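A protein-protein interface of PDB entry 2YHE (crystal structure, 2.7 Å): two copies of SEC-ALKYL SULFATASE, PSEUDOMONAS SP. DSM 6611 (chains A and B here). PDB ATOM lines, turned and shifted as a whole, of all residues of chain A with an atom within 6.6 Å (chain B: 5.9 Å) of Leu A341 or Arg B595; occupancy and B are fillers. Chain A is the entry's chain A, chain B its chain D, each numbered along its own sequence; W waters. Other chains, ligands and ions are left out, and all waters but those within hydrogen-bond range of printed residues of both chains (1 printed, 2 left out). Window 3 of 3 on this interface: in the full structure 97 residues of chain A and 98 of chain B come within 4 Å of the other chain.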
ATOM      1  N   GLN A 285      29.360  -7.783 -24.606  1.00  0.00           N
ATOM      2  CA  GLN A 285      28.804  -9.006 -24.010  1.00  0.00           C
ATOM      3  C   GLN A 285      29.950  -9.980 -23.884  1.00  0.00           C
ATOM      4  O   GLN A 285      30.421 -10.463 -24.908  1.00  0.00           O
ATOM      5  CB  GLN A 285      27.704  -9.633 -24.901  1.00  0.00           C
ATOM      6  CG  GLN A 285      27.298 -11.027 -24.423  1.00  0.00           C
ATOM      7  CD  GLN A 285      26.499 -11.830 -25.404  1.00  0.00           C
ATOM      8  OE1 GLN A 285      26.373 -11.484 -26.575  1.00  0.00           O
ATOM      9  NE2 GLN A 285      25.952 -12.945 -24.949  1.00  0.00           N
ATOM     10  N   LEU A 306      24.528  -5.986 -34.404  1.00  0.00           N
ATOM     11  CA  LEU A 306      25.253  -6.859 -33.512  1.00  0.00           C
ATOM     12  C   LEU A 306      26.493  -7.387 -34.209  1.00  0.00           C
ATOM     13  O   LEU A 306      26.402  -7.943 -35.307  1.00  0.00           O
ATOM     14  CB  LEU A 306      24.366  -8.016 -33.014  1.00  0.00           C
ATOM     15  CG  LEU A 306      24.994  -9.008 -32.019  1.00  0.00           C
ATOM     16  CD1 LEU A 306      25.451  -8.320 -30.717  1.00  0.00           C
ATOM     17  CD2 LEU A 306      24.054 -10.139 -31.765  1.00  0.00           C
ATOM     18  N   TYR A 336      25.948 -18.332 -24.800  1.00  0.00           N
ATOM     19  CA  TYR A 336      26.278 -16.959 -25.177  1.00  0.00           C
ATOM     20  C   TYR A 336      25.504 -16.556 -26.422  1.00  0.00           C
ATOM     21  O   TYR A 336      25.006 -15.438 -26.489  1.00  0.00           O
ATOM     22  CB  TYR A 336      27.782 -16.816 -25.420  1.00  0.00           C
ATOM     23  CG  TYR A 336      28.654 -17.000 -24.202  1.00  0.00           C
ATOM     24  CD1 TYR A 336      28.365 -16.347 -23.003  1.00  0.00           C
ATOM     25  CD2 TYR A 336      29.805 -17.782 -24.256  1.00  0.00           C
ATOM     26  CE1 TYR A 336      29.169 -16.511 -21.874  1.00  0.00           C
ATOM     27  CE2 TYR A 336      30.614 -17.961 -23.129  1.00  0.00           C
ATOM     28  CZ  TYR A 336      30.305 -17.304 -21.944  1.00  0.00           C
ATOM     29  OH  TYR A 336      31.130 -17.432 -20.845  1.00  0.00           O
ATOM     30  N   ILE A 337      25.394 -17.452 -27.406  1.00  0.00           N
ATOM     31  CA  ILE A 337      24.635 -17.161 -28.625  1.00  0.00           C
ATOM     32  C   ILE A 337      23.182 -16.864 -28.276  1.00  0.00           C
ATOM     33  O   ILE A 337      22.686 -15.815 -28.663  1.00  0.00           O
ATOM     34  CB  ILE A 337      24.778 -18.263 -29.698  1.00  0.00           C
ATOM     35  CG1 ILE A 337      26.220 -18.332 -30.217  1.00  0.00           C
ATOM     36  CG2 ILE A 337      23.791 -18.022 -30.865  1.00  0.00           C
ATOM     37  CD1 ILE A 337      26.560 -19.607 -30.995  1.00  0.00           C
ATOM     38  N   ASP A 338      22.539 -17.753 -27.473  1.00  0.00           N
ATOM     39  CA  ASP A 338      21.154 -17.615 -27.021  1.00  0.00           C
ATOM     40  C   ASP A 338      20.968 -16.317 -26.270  1.00  0.00           C
ATOM     41  O   ASP A 338      19.969 -15.633 -26.494  1.00  0.00           O
ATOM     42  CB  ASP A 338      20.759 -18.785 -26.124  1.00  0.00           C
ATOM     43  CG  ASP A 338      19.258 -19.048 -26.067  1.00  0.00           C
ATOM     44  OD1 ASP A 338      18.571 -18.793 -27.083  1.00  0.00           O
ATOM     45  OD2 ASP A 338      18.793 -19.616 -25.045  1.00  0.00           O
ATOM     46  N   ALA A 339      21.956 -15.954 -25.414  1.00  0.00           N
ATOM     47  CA  ALA A 339      21.922 -14.708 -24.665  1.00  0.00           C
ATOM     48  C   ALA A 339      21.893 -13.502 -25.632  1.00  0.00           C
ATOM     49  O   ALA A 339      21.128 -12.573 -25.375  1.00  0.00           O
ATOM     50  CB  ALA A 339      23.097 -14.622 -23.708  1.00  0.00           C
ATOM     51  N   SER A 340      22.653 -13.549 -26.768  1.00  0.00           N
ATOM     52  CA  SER A 340      22.659 -12.486 -27.789  1.00  0.00           C
ATOM     53  C   SER A 340      21.292 -12.441 -28.473  1.00  0.00           C
ATOM     54  O   SER A 340      20.766 -11.348 -28.713  1.00  0.00           O
ATOM     55  CB  SER A 340      23.702 -12.763 -28.864  1.00  0.00           C
ATOM     56  OG  SER A 340      24.986 -12.975 -28.315  1.00  0.00           O
ATOM     57  N   LEU A 341      20.721 -13.640 -28.793  1.00  0.00           N
ATOM     58  CA  LEU A 341      19.428 -13.774 -29.458  1.00  0.00           C
ATOM     59  C   LEU A 341      18.298 -13.192 -28.608  1.00  0.00           C
ATOM     60  O   LEU A 341      17.404 -12.522 -29.140  1.00  0.00           O
ATOM     61  CB  LEU A 341      19.156 -15.238 -29.828  1.00  0.00           C
ATOM     62  CG  LEU A 341      17.807 -15.563 -30.488  1.00  0.00           C
ATOM     63  CD1 LEU A 341      17.610 -14.801 -31.775  1.00  0.00           C
ATOM     64  CD2 LEU A 341      17.693 -17.025 -30.766  1.00  0.00           C
ATOM     65  N   GLU A 342      18.354 -13.451 -27.282  1.00  0.00           N
ATOM     66  CA  GLU A 342      17.375 -12.920 -26.363  1.00  0.00           C
ATOM     67  C   GLU A 342      17.568 -11.404 -26.183  1.00  0.00           C
ATOM     68  O   GLU A 342      16.633 -10.640 -26.469  1.00  0.00           O
ATOM     69  CB  GLU A 342      17.404 -13.660 -25.031  1.00  0.00           C
ATOM     70  CG  GLU A 342      16.214 -13.310 -24.158  1.00  0.00           C
ATOM     71  CD  GLU A 342      16.153 -13.968 -22.802  1.00  0.00           C
ATOM     72  OE1 GLU A 342      17.073 -14.745 -22.458  1.00  0.00           O
ATOM     73  OE2 GLU A 342      15.198 -13.654 -22.057  1.00  0.00           O
ATOM     74  N   LYS A 343      18.785 -10.985 -25.749  1.00  0.00           N
ATOM     75  CA  LYS A 343      19.113  -9.597 -25.461  1.00  0.00           C
ATOM     76  C   LYS A 343      19.093  -8.631 -26.646  1.00  0.00           C
ATOM     77  O   LYS A 343      18.793  -7.453 -26.436  1.00  0.00           O
ATOM     78  CB  LYS A 343      20.425  -9.483 -24.659  1.00  0.00           C
ATOM     79  CG  LYS A 343      20.442  -8.279 -23.706  1.00  0.00           C
ATOM     80  CD  LYS A 343      21.551  -8.344 -22.658  1.00  0.00           C
ATOM     81  CE  LYS A 343      21.363  -7.382 -21.501  1.00  0.00           C
ATOM     82  NZ  LYS A 343      21.501  -5.945 -21.885  1.00  0.00           N
ATOM     83  N   TYR A 344      19.437  -9.088 -27.871  1.00  0.00           N
ATOM     84  CA  TYR A 344      19.562  -8.172 -29.019  1.00  0.00           C
ATOM     85  C   TYR A 344      18.813  -8.567 -30.257  1.00  0.00           C
ATOM     86  O   TYR A 344      18.673  -7.741 -31.149  1.00  0.00           O
ATOM     87  CB  TYR A 344      21.047  -7.965 -29.401  1.00  0.00           C
ATOM     88  CG  TYR A 344      21.973  -7.708 -28.239  1.00  0.00           C
ATOM     89  CD1 TYR A 344      21.858  -6.555 -27.477  1.00  0.00           C
ATOM     90  CD2 TYR A 344      22.965  -8.616 -27.904  1.00  0.00           C
ATOM     91  CE1 TYR A 344      22.720  -6.300 -26.416  1.00  0.00           C
ATOM     92  CE2 TYR A 344      23.841  -8.375 -26.847  1.00  0.00           C
ATOM     93  CZ  TYR A 344      23.712  -7.214 -26.103  1.00  0.00           C
ATOM     94  OH  TYR A 344      24.567  -6.953 -25.057  1.00  0.00           O
ATOM     95  N   GLY A 345      18.376  -9.808 -30.329  1.00  0.00           N
ATOM     96  CA  GLY A 345      17.669 -10.332 -31.492  1.00  0.00           C
ATOM     97  C   GLY A 345      16.507  -9.507 -32.010  1.00  0.00           C
ATOM     98  O   GLY A 345      16.255  -9.461 -33.219  1.00  0.00           O
ATOM     99  N   ASP A 346      15.782  -8.869 -31.096  1.00  0.00           N
ATOM    100  CA  ASP A 346      14.616  -8.081 -31.465  1.00  0.00           C
ATOM    101  C   ASP A 346      14.958  -6.630 -31.789  1.00  0.00           C
ATOM    102  O   ASP A 346      14.120  -5.914 -32.326  1.00  0.00           O
ATOM    103  CB  ASP A 346      13.491  -8.228 -30.427  1.00  0.00           C
ATOM    104  CG  ASP A 346      12.995  -9.653 -30.256  1.00  0.00           C
ATOM    105  OD1 ASP A 346      12.768 -10.341 -31.280  1.00  0.00           O
ATOM    106  OD2 ASP A 346      12.824 -10.075 -29.111  1.00  0.00           O
ATOM    107  N   VAL A 365      18.439 -12.766 -39.118  1.00  0.00           N
ATOM    108  CA  VAL A 365      19.385 -12.769 -38.002  1.00  0.00           C
ATOM    109  C   VAL A 365      18.890 -13.622 -36.843  1.00  0.00           C
ATOM    110  O   VAL A 365      19.689 -14.349 -36.247  1.00  0.00           O
ATOM    111  CB  VAL A 365      20.038 -11.407 -37.578  1.00  0.00           C
ATOM    112  CG1 VAL A 365      19.914 -10.327 -38.654  1.00  0.00           C
ATOM    113  CG2 VAL A 365      19.512 -10.914 -36.251  1.00  0.00           C
ATOM    114  N   ARG A 366      17.577 -13.584 -36.561  1.00  0.00           N
ATOM    115  CA  ARG A 366      16.991 -14.370 -35.480  1.00  0.00           C
ATOM    116  C   ARG A 366      17.036 -15.854 -35.784  1.00  0.00           C
ATOM    117  O   ARG A 366      17.329 -16.645 -34.883  1.00  0.00           O
ATOM    118  CB  ARG A 366      15.577 -13.892 -35.106  1.00  0.00           C
ATOM    119  CG  ARG A 366      15.558 -12.612 -34.275  1.00  0.00           C
ATOM    120  CD  ARG A 366      14.163 -12.171 -33.878  1.00  0.00           C
ATOM    121  NE  ARG A 366      13.352 -11.776 -35.034  1.00  0.00           N
ATOM    122  CZ  ARG A 366      13.334 -10.543 -35.544  1.00  0.00           C
ATOM    123  NH1 ARG A 366      14.089  -9.584 -35.017  1.00  0.00           N
ATOM    124  NH2 ARG A 366      12.582 -10.268 -36.599  1.00  0.00           N
ATOM    125  N   THR A 367      16.821 -16.231 -37.057  1.00  0.00           N
ATOM    126  CA  THR A 367      16.870 -17.632 -37.487  1.00  0.00           C
ATOM    127  C   THR A 367      18.307 -18.160 -37.389  1.00  0.00           C
ATOM    128  O   THR A 367      18.539 -19.252 -36.846  1.00  0.00           O
ATOM    129  CB  THR A 367      16.266 -17.788 -38.877  1.00  0.00           C
ATOM    130  OG1 THR A 367      14.927 -17.337 -38.836  1.00  0.00           O
ATOM    131  CG2 THR A 367      16.252 -19.245 -39.348  1.00  0.00           C
ATOM    132  N   LEU A 369      20.987 -16.987 -35.535  1.00  0.00           N
ATOM    133  CA  LEU A 369      21.416 -17.150 -34.146  1.00  0.00           C
ATOM    134  C   LEU A 369      20.809 -18.393 -33.497  1.00  0.00           C
ATOM    135  O   LEU A 369      21.534 -19.142 -32.839  1.00  0.00           O
ATOM    136  CB  LEU A 369      21.103 -15.896 -33.321  1.00  0.00           C
ATOM    137  CG  LEU A 369      21.849 -14.600 -33.674  1.00  0.00           C
ATOM    138  CD1 LEU A 369      21.381 -13.492 -32.821  1.00  0.00           C
ATOM    139  CD2 LEU A 369      23.359 -14.735 -33.508  1.00  0.00           C
ATOM    140  N   ALA A 370      19.506 -18.651 -33.723  1.00  0.00           N
ATOM    141  CA  ALA A 370      18.836 -19.844 -33.176  1.00  0.00           C
ATOM    142  C   ALA A 370      19.498 -21.101 -33.724  1.00  0.00           C
ATOM    143  O   ALA A 370      19.738 -22.054 -32.980  1.00  0.00           O
ATOM    144  CB  ALA A 370      17.353 -19.832 -33.528  1.00  0.00           C
ATOM    145  N   ASP A 371      19.825 -21.082 -35.027  1.00  0.00           N
ATOM    146  CA  ASP A 371      20.467 -22.190 -35.722  1.00  0.00           C
ATOM    147  C   ASP A 371      21.884 -22.398 -35.170  1.00  0.00           C
ATOM    148  O   ASP A 371      22.251 -23.532 -34.859  1.00  0.00           O
ATOM    149  CB  ASP A 371      20.465 -21.931 -37.246  1.00  0.00           C
ATOM    150  CG  ASP A 371      19.148 -22.197 -37.945  1.00  0.00           C
ATOM    151  OD1 ASP A 371      18.317 -22.915 -37.382  1.00  0.00           O
ATOM    152  OD2 ASP A 371      18.983 -21.747 -39.094  1.00  0.00           O
ATOM    153  N   ARG A 373      23.155 -21.468 -32.152  1.00  0.00           N
ATOM    154  CA  ARG A 373      22.979 -21.965 -30.789  1.00  0.00           C
ATOM    155  C   ARG A 373      22.719 -23.452 -30.782  1.00  0.00           C
ATOM    156  O   ARG A 373      23.412 -24.200 -30.076  1.00  0.00           O
ATOM    157  CB  ARG A 373      21.819 -21.227 -30.141  1.00  0.00           C
ATOM    158  CG  ARG A 373      21.476 -21.736 -28.766  1.00  0.00           C
ATOM    159  CD  ARG A 373      20.028 -21.478 -28.434  1.00  0.00           C
ATOM    160  NE  ARG A 373      19.107 -22.110 -29.375  1.00  0.00           N
ATOM    161  CZ  ARG A 373      17.905 -21.641 -29.668  1.00  0.00           C
ATOM    162  NH1 ARG A 373      17.460 -20.538 -29.093  1.00  0.00           N
ATOM    163  NH2 ARG A 373      17.136 -22.272 -30.532  1.00  0.00           N
ATOM    164  N   ASP B 582      11.267 -19.013 -13.294  1.00  0.00           N
ATOM    165  CA  ASP B 582      10.665 -19.349 -14.584  1.00  0.00           C
ATOM    166  C   ASP B 582      11.713 -19.904 -15.534  1.00  0.00           C
ATOM    167  O   ASP B 582      12.770 -19.286 -15.705  1.00  0.00           O
ATOM    168  CB  ASP B 582      10.023 -18.107 -15.225  1.00  0.00           C
ATOM    169  CG  ASP B 582       8.783 -17.592 -14.535  1.00  0.00           C
ATOM    170  OD1 ASP B 582       7.983 -18.424 -14.042  1.00  0.00           O
ATOM    171  OD2 ASP B 582       8.560 -16.366 -14.570  1.00  0.00           O
ATOM    172  N   ILE B 583      11.431 -21.055 -16.151  1.00  0.00           N
ATOM    173  CA  ILE B 583      12.337 -21.614 -17.148  1.00  0.00           C
ATOM    174  C   ILE B 583      11.616 -21.859 -18.480  1.00  0.00           C
ATOM    175  O   ILE B 583      10.576 -22.517 -18.508  1.00  0.00           O
ATOM    176  CB  ILE B 583      13.302 -22.769 -16.675  1.00  0.00           C
ATOM    177  CG1 ILE B 583      13.166 -24.048 -17.453  1.00  0.00           C
ATOM    178  CG2 ILE B 583      13.500 -22.971 -15.164  1.00  0.00           C
ATOM    179  CD1 ILE B 583      13.981 -24.048 -18.646  1.00  0.00           C
ATOM    180  N   ALA B 584      12.151 -21.282 -19.569  1.00  0.00           N
ATOM    181  CA  ALA B 584      11.593 -21.456 -20.913  1.00  0.00           C
ATOM    182  C   ALA B 584      12.406 -22.528 -21.630  1.00  0.00           C
ATOM    183  O   ALA B 584      13.576 -22.316 -21.932  1.00  0.00           O
ATOM    184  CB  ALA B 584      11.615 -20.133 -21.687  1.00  0.00           C
ATOM    185  N   LEU B 585      11.806 -23.707 -21.815  1.00  0.00           N
ATOM    186  CA  LEU B 585      12.447 -24.852 -22.475  1.00  0.00           C
ATOM    187  C   LEU B 585      12.112 -24.847 -23.928  1.00  0.00           C
ATOM    188  O   LEU B 585      10.947 -24.689 -24.276  1.00  0.00           O
ATOM    189  CB  LEU B 585      11.955 -26.189 -21.907  1.00  0.00           C
ATOM    190  CG  LEU B 585      12.814 -26.957 -20.930  1.00  0.00           C
ATOM    191  CD1 LEU B 585      12.473 -28.430 -21.023  1.00  0.00           C
ATOM    192  CD2 LEU B 585      14.280 -26.801 -21.233  1.00  0.00           C
ATOM    193  N   THR B 586      13.118 -25.028 -24.791  1.00  0.00           N
ATOM    194  CA  THR B 586      12.887 -25.112 -26.226  1.00  0.00           C
ATOM    195  C   THR B 586      13.554 -26.326 -26.829  1.00  0.00           C
ATOM    196  O   THR B 586      14.750 -26.546 -26.641  1.00  0.00           O
ATOM    197  CB  THR B 586      12.975 -23.743 -26.989  1.00  0.00           C
ATOM    198  OG1 THR B 586      13.550 -23.905 -28.287  1.00  0.00           O
ATOM    199  CG2 THR B 586      13.733 -22.676 -26.246  1.00  0.00           C
ATOM    200  N   THR B 593      17.433 -26.667 -25.374  1.00  0.00           N
ATOM    201  CA  THR B 593      18.013 -25.462 -24.779  1.00  0.00           C
ATOM    202  C   THR B 593      16.992 -24.829 -23.803  1.00  0.00           C
ATOM    203  O   THR B 593      15.772 -25.060 -23.904  1.00  0.00           O
ATOM    204  CB  THR B 593      18.537 -24.501 -25.823  1.00  0.00           C
ATOM    205  OG1 THR B 593      17.468 -24.097 -26.678  1.00  0.00           O
ATOM    206  CG2 THR B 593      19.677 -25.086 -26.615  1.00  0.00           C
ATOM    207  N   GLN B 594      17.506 -24.052 -22.843  1.00  0.00           N
ATOM    208  CA  GLN B 594      16.668 -23.421 -21.823  1.00  0.00           C
ATOM    209  C   GLN B 594      17.076 -21.986 -21.548  1.00  0.00           C
ATOM    210  O   GLN B 594      18.236 -21.612 -21.760  1.00  0.00           O
ATOM    211  CB  GLN B 594      16.721 -24.236 -20.517  1.00  0.00           C
ATOM    212  CG  GLN B 594      18.129 -24.621 -20.083  1.00  0.00           C
ATOM    213  CD  GLN B 594      18.281 -24.881 -18.628  1.00  0.00           C
ATOM    214  OE1 GLN B 594      17.568 -24.324 -17.785  1.00  0.00           O
ATOM    215  NE2 GLN B 594      19.267 -25.694 -18.295  1.00  0.00           N
ATOM    216  N   ARG B 595      16.119 -21.199 -21.067  1.00  0.00           N
ATOM    217  CA  ARG B 595      16.330 -19.815 -20.664  1.00  0.00           C
ATOM    218  C   ARG B 595      15.813 -19.665 -19.235  1.00  0.00           C
ATOM    219  O   ARG B 595      14.662 -19.999 -18.958  1.00  0.00           O
ATOM    220  CB  ARG B 595      15.647 -18.812 -21.627  1.00  0.00           C
ATOM    221  CG  ARG B 595      16.355 -18.687 -22.953  1.00  0.00           C
ATOM    222  CD  ARG B 595      15.685 -17.665 -23.833  1.00  0.00           C
ATOM    223  NE  ARG B 595      16.204 -17.698 -25.200  1.00  0.00           N
ATOM    224  CZ  ARG B 595      15.693 -17.006 -26.209  1.00  0.00           C
ATOM    225  NH1 ARG B 595      14.641 -16.224 -26.020  1.00  0.00           N
ATOM    226  NH2 ARG B 595      16.222 -17.098 -27.416  1.00  0.00           N
ATOM    227  N   VAL B 596      16.681 -19.218 -18.338  1.00  0.00           N
ATOM    228  CA  VAL B 596      16.361 -18.993 -16.930  1.00  0.00           C
ATOM    229  C   VAL B 596      15.813 -17.574 -16.775  1.00  0.00           C
ATOM    230  O   VAL B 596      16.350 -16.632 -17.358  1.00  0.00           O
ATOM    231  CB  VAL B 596      17.595 -19.254 -15.992  1.00  0.00           C
ATOM    232  CG1 VAL B 596      17.198 -19.193 -14.525  1.00  0.00           C
ATOM    233  CG2 VAL B 596      18.262 -20.597 -16.297  1.00  0.00           C
ATOM    234  N   GLY B 597      14.741 -17.449 -16.005  1.00  0.00           N
ATOM    235  CA  GLY B 597      14.102 -16.174 -15.709  1.00  0.00           C
ATOM    236  C   GLY B 597      13.144 -15.647 -16.763  1.00  0.00           C
ATOM    237  O   GLY B 597      12.609 -14.546 -16.603  1.00  0.00           O
ATOM    238  N   SER B 598      12.887 -16.403 -17.841  1.00  0.00           N
ATOM    239  CA  SER B 598      11.947 -15.933 -18.860  1.00  0.00           C
ATOM    240  C   SER B 598      10.935 -16.998 -19.250  1.00  0.00           C
ATOM    241  O   SER B 598      11.125 -18.179 -18.925  1.00  0.00           O
ATOM    242  CB  SER B 598      12.678 -15.379 -20.079  1.00  0.00           C
ATOM    243  OG  SER B 598      13.367 -16.370 -20.824  1.00  0.00           O
HETATM  244  O   HOH W   1      16.768 -21.480 -25.526  1.00  0.00           O
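Among the printed residues, merely in contact across the chains: Glu A342 with Arg B595, Leu A341 with Arg B595, Arg A373 with Thr B593 and Asp A338 with Gln B594.
No position is printed for both chains.
Water W1 lies within hydrogen-bond range of the side-chain carboxylate (OD2) of Asp A338 and the side-chain hydroxyl (OG1) of Thr B593.
The side-chain carboxylate of Asp A338 lies within salt-bridge range of the guanidinium group of Arg B595, 2.9 Å away. The side-chain carboxylate (OE2) of Glu A342 sits close to the side-chain hydroxyl (OG) of Ser B598 (3.5 Å).
Of chain B, only Arg B595 comes within 4 Å of Leu A341. Printed residues of chain A within 4 Å of Arg B595: Asp A338, Leu A341 and Glu A342. Printed residues of chain B within 4 Å of Glu A342: Arg B595 and Ser B598. Of the printed residues of chain A, Thr B593 touches Arg A373. Of the printed residues of chain B, Arg A373 touches Thr B593. Of the printed residues of chain A, Gln B594 touches Asp A338. The nearest printed residue of chain B that does not touch Leu A341 is Thr B593 (8.2 Å). The nearest residue of chain A that does not touch Arg B595 is Arg A373 (4.02 Å).
N of Thr B586 lies within hydrogen-bond range of O of Thr B593, at 2.8 Å. NH1 of Arg A373 lies within salt-bridge range of OD1 of Asp A338 (2.9 Å). The backbone carbonyl oxygen (O) of Arg B595 lies within hydrogen-bond range of the backbone NH (N) of Ala B584 (2.9 Å). The backbone carbonyl oxygen (O) of Ser B598 sits at hydrogen-bond distance from the backbone NH (N) of Ala B584 (3.3 Å).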
